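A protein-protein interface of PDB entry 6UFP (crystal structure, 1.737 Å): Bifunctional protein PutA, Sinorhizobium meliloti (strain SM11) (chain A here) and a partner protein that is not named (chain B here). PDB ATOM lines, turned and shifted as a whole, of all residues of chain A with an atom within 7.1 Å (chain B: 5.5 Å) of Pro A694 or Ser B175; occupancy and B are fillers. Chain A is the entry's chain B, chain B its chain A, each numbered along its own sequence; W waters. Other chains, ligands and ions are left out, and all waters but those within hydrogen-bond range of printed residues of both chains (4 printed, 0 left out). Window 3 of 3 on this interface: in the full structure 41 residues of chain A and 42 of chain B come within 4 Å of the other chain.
The guanidinium group of Arg B172 lies within hydrogen-bond range of the backbone carbonyl oxygen of Val A1039 (3.0 Å).
Of the 9 printed residues of chain B, 4 touch a printed residue of chain A. Printed residues of chain B that touch a printed residue of chain A: Thr B171, Arg B172, Ser B175 and Arg B176. Along chain A the printed residues that touch a printed residue of chain B span positions 691 to 1039.
Of the printed residues of chain B, Pro A694 touches Ser B175. Of chain A, only Gly A693 (3.5 Å), Pro A694 (3.7 Å) and His A696 (3.8 Å) come within 4 Å of Ser B175. Printed residues of chain B within 4 Å of Gly A693: Ser B175 (3.5 Å). Of the printed residues of chain B, Leu A692 touches Arg B176 (3.9 Å). Of the printed residues of chain A, Arg B172 touches Val A1039 (3.0 Å). Of the printed residues of chain B, Thr A691 touches Arg B176 (3.9 Å). Of the printed residues of chain A, Arg B176 touches Thr A691 (3.9 Å) and Leu A692 (3.9 Å). The nearest residue of chain B that does not touch Pro A694 is Arg B176 (4.1 Å). The nearest residue of chain A that does not touch Ser B175 is Gly A695 (5.0 Å).
O of Thr B171 lies close to OG of Ser B175, at 3.3 Å. N of Gly A693 is in hydrogen-bond range of ND1 of His A696 (3.0 Å).
Thr A691 touches Arg B176 (N to CD, 3.9 Å). CG of Arg B176 touches O of Leu A692, at 3.9 Å. O of Ser B175 touches CA of Gly A693 (3.5 Å). CD of Pro A694 touches O of Ser B175 (3.7 Å). CB of Ser B175 touches CE1 of His A696, 3.8 Å away. CG2 of Thr B171 touches CG2 of Val A1039, 3.8 Å away.
Water W4 lies within hydrogen-bond range of the backbone carbonyl oxygen (O) of Thr A691 and the backbone carbonyl oxygen (O) of Arg B172. Water W2 bridges O of Ser B175 and N of Gly A695. Water W3 bridges the side-chain hydroxyl of Ser B175 and a ring nitrogen (NE2) of His A696. Water W1 lies within hydrogen-bond range of OG of Ser B175 (3.2 Å) and NE2 of His A696 (3.5 Å).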
ATOM      1  N   PRO A 634     -20.686 -16.849   4.142  1.00  0.00           N
ATOM      2  CA  PRO A 634     -21.842 -15.936   4.209  1.00  0.00           C
ATOM      3  C   PRO A 634     -21.754 -14.763   3.245  1.00  0.00           C
ATOM      4  O   PRO A 634     -22.761 -14.415   2.620  1.00  0.00           O
ATOM      5  CB  PRO A 634     -21.829 -15.456   5.666  1.00  0.00           C
ATOM      6  CG  PRO A 634     -21.095 -16.536   6.433  1.00  0.00           C
ATOM      7  CD  PRO A 634     -20.161 -17.218   5.476  1.00  0.00           C
ATOM      8  N   THR A 691     -23.272  -9.755  10.299  1.00  0.00           N
ATOM      9  CA  THR A 691     -23.406 -10.602  11.489  1.00  0.00           C
ATOM     10  C   THR A 691     -22.839 -12.018  11.398  1.00  0.00           C
ATOM     11  O   THR A 691     -22.312 -12.516  12.398  1.00  0.00           O
ATOM     12  CB  THR A 691     -24.893 -10.706  11.890  1.00  0.00           C
ATOM     13  OG1 THR A 691     -25.662 -11.276  10.817  1.00  0.00           O
ATOM     14  CG2 THR A 691     -25.450  -9.342  12.248  1.00  0.00           C
ATOM     15  N   LEU A 692     -22.985 -12.713  10.274  1.00  0.00           N
ATOM     16  CA  LEU A 692     -22.819 -14.166  10.310  1.00  0.00           C
ATOM     17  C   LEU A 692     -21.352 -14.600  10.194  1.00  0.00           C
ATOM     18  O   LEU A 692     -20.620 -14.160   9.300  1.00  0.00           O
ATOM     19  CB  LEU A 692     -23.659 -14.827   9.214  1.00  0.00           C
ATOM     20  CG  LEU A 692     -25.181 -14.704   9.365  1.00  0.00           C
ATOM     21  CD1 LEU A 692     -25.909 -15.602   8.359  1.00  0.00           C
ATOM     22  CD2 LEU A 692     -25.626 -15.030  10.788  1.00  0.00           C
ATOM     23  N   GLY A 693     -20.938 -15.474  11.108  1.00  0.00           N
ATOM     24  CA  GLY A 693     -19.590 -15.997  11.140  1.00  0.00           C
ATOM     25  C   GLY A 693     -19.609 -17.509  11.272  1.00  0.00           C
ATOM     26  O   GLY A 693     -20.673 -18.140  11.262  1.00  0.00           O
ATOM     27  N   PRO A 694     -18.427 -18.118  11.418  1.00  0.00           N
ATOM     28  CA  PRO A 694     -18.359 -19.592  11.402  1.00  0.00           C
ATOM     29  C   PRO A 694     -19.142 -20.258  12.517  1.00  0.00           C
ATOM     30  O   PRO A 694     -19.593 -21.399  12.349  1.00  0.00           O
ATOM     31  CB  PRO A 694     -16.851 -19.878  11.516  1.00  0.00           C
ATOM     32  CG  PRO A 694     -16.240 -18.599  12.035  1.00  0.00           C
ATOM     33  CD  PRO A 694     -17.100 -17.485  11.533  1.00  0.00           C
ATOM     34  N   GLY A 695     -19.331 -19.587  13.649  1.00  0.00           N
ATOM     35  CA  GLY A 695     -20.061 -20.171  14.751  1.00  0.00           C
ATOM     36  C   GLY A 695     -21.567 -20.117  14.651  1.00  0.00           C
ATOM     37  O   GLY A 695     -22.255 -20.645  15.530  1.00  0.00           O
ATOM     38  N   HIS A 696     -22.107 -19.492  13.604  1.00  0.00           N
ATOM     39  CA  HIS A 696     -23.551 -19.359  13.430  1.00  0.00           C
ATOM     40  C   HIS A 696     -24.012 -20.385  12.399  1.00  0.00           C
ATOM     41  O   HIS A 696     -24.301 -20.073  11.247  1.00  0.00           O
ATOM     42  CB  HIS A 696     -23.903 -17.935  13.025  1.00  0.00           C
ATOM     43  CG  HIS A 696     -23.364 -16.918  13.973  1.00  0.00           C
ATOM     44  ND1 HIS A 696     -22.405 -16.000  13.613  1.00  0.00           N
ATOM     45  CD2 HIS A 696     -23.606 -16.719  15.289  1.00  0.00           C
ATOM     46  CE1 HIS A 696     -22.097 -15.257  14.661  1.00  0.00           C
ATOM     47  NE2 HIS A 696     -22.804 -15.683  15.695  1.00  0.00           N
ATOM     48  N   GLY A 697     -24.097 -21.633  12.845  1.00  0.00           N
ATOM     49  CA  GLY A 697     -24.358 -22.733  11.950  1.00  0.00           C
ATOM     50  C   GLY A 697     -25.800 -22.806  11.494  1.00  0.00           C
ATOM     51  O   GLY A 697     -26.737 -22.469  12.226  1.00  0.00           O
ATOM     52  N   PRO A 698     -26.006 -23.262  10.264  1.00  0.00           N
ATOM     53  CA  PRO A 698     -27.370 -23.347   9.734  1.00  0.00           C
ATOM     54  C   PRO A 698     -28.165 -24.447  10.417  1.00  0.00           C
ATOM     55  O   PRO A 698     -27.623 -25.362  11.036  1.00  0.00           O
ATOM     56  CB  PRO A 698     -27.158 -23.664   8.252  1.00  0.00           C
ATOM     57  CG  PRO A 698     -25.844 -24.370   8.225  1.00  0.00           C
ATOM     58  CD  PRO A 698     -25.003 -23.682   9.279  1.00  0.00           C
ATOM     59  N   PRO A1038     -26.610 -14.628  16.177  1.00  0.00           N
ATOM     60  CA  PRO A1038     -25.616 -13.565  16.360  1.00  0.00           C
ATOM     61  C   PRO A1038     -26.217 -12.375  17.099  1.00  0.00           C
ATOM     62  O   PRO A1038     -27.407 -12.310  17.375  1.00  0.00           O
ATOM     63  CB  PRO A1038     -25.257 -13.167  14.927  1.00  0.00           C
ATOM     64  CG  PRO A1038     -26.538 -13.378  14.182  1.00  0.00           C
ATOM     65  CD  PRO A1038     -27.154 -14.644  14.804  1.00  0.00           C
ATOM     66  N   VAL A1039     -25.352 -11.405  17.375  1.00  0.00           N
ATOM     67  CA  VAL A1039     -25.759 -10.123  17.944  1.00  0.00           C
ATOM     68  C   VAL A1039     -26.106  -9.196  16.783  1.00  0.00           C
ATOM     69  O   VAL A1039     -25.201  -8.788  16.044  1.00  0.00           O
ATOM     70  CB  VAL A1039     -24.641  -9.522  18.805  1.00  0.00           C
ATOM     71  CG1 VAL A1039     -25.108  -8.177  19.429  1.00  0.00           C
ATOM     72  CG2 VAL A1039     -24.215 -10.519  19.872  1.00  0.00           C
ATOM     73  N   LEU B 170     -18.259  -5.554  19.966  1.00  0.00           N
ATOM     74  CA  LEU B 170     -17.036  -6.348  20.044  1.00  0.00           C
ATOM     75  C   LEU B 170     -17.342  -7.836  19.899  1.00  0.00           C
ATOM     76  O   LEU B 170     -16.618  -8.556  19.203  1.00  0.00           O
ATOM     77  CB  LEU B 170     -16.310  -6.054  21.355  1.00  0.00           C
ATOM     78  CG  LEU B 170     -14.963  -6.785  21.477  1.00  0.00           C
ATOM     79  CD1 LEU B 170     -14.017  -6.401  20.350  1.00  0.00           C
ATOM     80  CD2 LEU B 170     -14.335  -6.498  22.837  1.00  0.00           C
ATOM     81  N   THR B 171     -18.409  -8.306  20.551  1.00  0.00           N
ATOM     82  CA  THR B 171     -18.875  -9.677  20.363  1.00  0.00           C
ATOM     83  C   THR B 171     -19.185  -9.940  18.895  1.00  0.00           C
ATOM     84  O   THR B 171     -18.726 -10.933  18.314  1.00  0.00           O
ATOM     85  CB  THR B 171     -20.114  -9.926  21.235  1.00  0.00           C
ATOM     86  OG1 THR B 171     -19.771  -9.776  22.617  1.00  0.00           O
ATOM     87  CG2 THR B 171     -20.706 -11.308  20.997  1.00  0.00           C
ATOM     88  N   ARG B 172     -19.922  -9.024  18.263  1.00  0.00           N
ATOM     89  CA  ARG B 172     -20.298  -9.207  16.862  1.00  0.00           C
ATOM     90  C   ARG B 172     -19.063  -9.307  15.965  1.00  0.00           C
ATOM     91  O   ARG B 172     -18.966 -10.212  15.122  1.00  0.00           O
ATOM     92  CB  ARG B 172     -21.218  -8.059  16.413  1.00  0.00           C
ATOM     93  CG  ARG B 172     -21.846  -8.268  15.027  1.00  0.00           C
ATOM     94  CD  ARG B 172     -22.623  -7.031  14.544  1.00  0.00           C
ATOM     95  NE  ARG B 172     -23.478  -6.439  15.576  1.00  0.00           N
ATOM     96  CZ  ARG B 172     -23.205  -5.309  16.231  1.00  0.00           C
ATOM     97  NH1 ARG B 172     -24.053  -4.856  17.152  1.00  0.00           N
ATOM     98  NH2 ARG B 172     -22.080  -4.637  15.986  1.00  0.00           N
ATOM     99  N   LEU B 173     -18.095  -8.401  16.139  1.00  0.00           N
ATOM    100  CA  LEU B 173     -16.975  -8.360  15.206  1.00  0.00           C
ATOM    101  C   LEU B 173     -16.045  -9.557  15.398  1.00  0.00           C
ATOM    102  O   LEU B 173     -15.522 -10.098  14.419  1.00  0.00           O
ATOM    103  CB  LEU B 173     -16.224  -7.030  15.336  1.00  0.00           C
ATOM    104  CG  LEU B 173     -15.239  -6.730  16.467  1.00  0.00           C
ATOM    105  CD1 LEU B 173     -13.815  -7.112  16.061  1.00  0.00           C
ATOM    106  CD2 LEU B 173     -15.275  -5.260  16.851  1.00  0.00           C
ATOM    107  N   ILE B 174     -15.868 -10.017  16.638  1.00  0.00           N
ATOM    108  CA  ILE B 174     -15.040 -11.200  16.867  1.00  0.00           C
ATOM    109  C   ILE B 174     -15.744 -12.440  16.336  1.00  0.00           C
ATOM    110  O   ILE B 174     -15.130 -13.296  15.682  1.00  0.00           O
ATOM    111  CB  ILE B 174     -14.699 -11.334  18.363  1.00  0.00           C
ATOM    112  CG1 ILE B 174     -13.743 -10.217  18.784  1.00  0.00           C
ATOM    113  CG2 ILE B 174     -14.097 -12.719  18.670  1.00  0.00           C
ATOM    114  CD1 ILE B 174     -13.591 -10.084  20.271  1.00  0.00           C
ATOM    115  N   SER B 175     -17.050 -12.545  16.585  1.00  0.00           N
ATOM    116  CA  SER B 175     -17.800 -13.696  16.096  1.00  0.00           C
ATOM    117  C   SER B 175     -17.819 -13.742  14.576  1.00  0.00           C
ATOM    118  O   SER B 175     -17.957 -14.817  13.985  1.00  0.00           O
ATOM    119  CB  SER B 175     -19.228 -13.673  16.637  1.00  0.00           C
ATOM    120  OG  SER B 175     -19.283 -14.140  17.969  1.00  0.00           O
ATOM    121  N   ARG B 176     -17.692 -12.591  13.929  1.00  0.00           N
ATOM    122  CA  ARG B 176     -17.714 -12.515  12.474  1.00  0.00           C
ATOM    123  C   ARG B 176     -16.340 -12.765  11.856  1.00  0.00           C
ATOM    124  O   ARG B 176     -16.216 -13.556  10.913  1.00  0.00           O
ATOM    125  CB  ARG B 176     -18.242 -11.138  12.048  1.00  0.00           C
ATOM    126  CG  ARG B 176     -18.714 -11.034  10.612  1.00  0.00           C
ATOM    127  CD  ARG B 176     -19.406  -9.685  10.366  1.00  0.00           C
ATOM    128  NE  ARG B 176     -18.491  -8.551  10.448  1.00  0.00           N
ATOM    129  CZ  ARG B 176     -18.589  -7.531  11.314  1.00  0.00           C
ATOM    130  NH1 ARG B 176     -19.580  -7.451  12.210  1.00  0.00           N
ATOM    131  NH2 ARG B 176     -17.681  -6.567  11.275  1.00  0.00           N
ATOM    132  N   CYS B 177     -15.294 -12.137  12.398  1.00  0.00           N
ATOM    133  CA  CYS B 177     -13.983 -12.109  11.761  1.00  0.00           C
ATOM    134  C   CYS B 177     -12.862 -12.768  12.551  1.00  0.00           C
ATOM    135  O   CYS B 177     -11.790 -12.984  11.982  1.00  0.00           O
ATOM    136  CB  CYS B 177     -13.563 -10.660  11.462  1.00  0.00           C
ATOM    137  SG  CYS B 177     -14.776  -9.747  10.494  1.00  0.00           S
ATOM    138  N   GLY B 178     -13.051 -13.049  13.835  1.00  0.00           N
ATOM    139  CA  GLY B 178     -12.098 -13.899  14.539  1.00  0.00           C
ATOM    140  C   GLY B 178     -10.725 -13.288  14.790  1.00  0.00           C
ATOM    141  O   GLY B 178     -10.534 -12.076  14.848  1.00  0.00           O
HETATM  142  O   HOH W   1     -19.969 -17.145  17.101  1.00  0.00           O
HETATM  143  O   HOH W   2     -18.633 -17.235  14.949  1.00  0.00           O
HETATM  144  O   HOH W   3     -22.109 -14.428  18.551  1.00  0.00           O
HETATM  145  O   HOH W   4     -21.097 -11.963  14.704  1.00  0.00           O
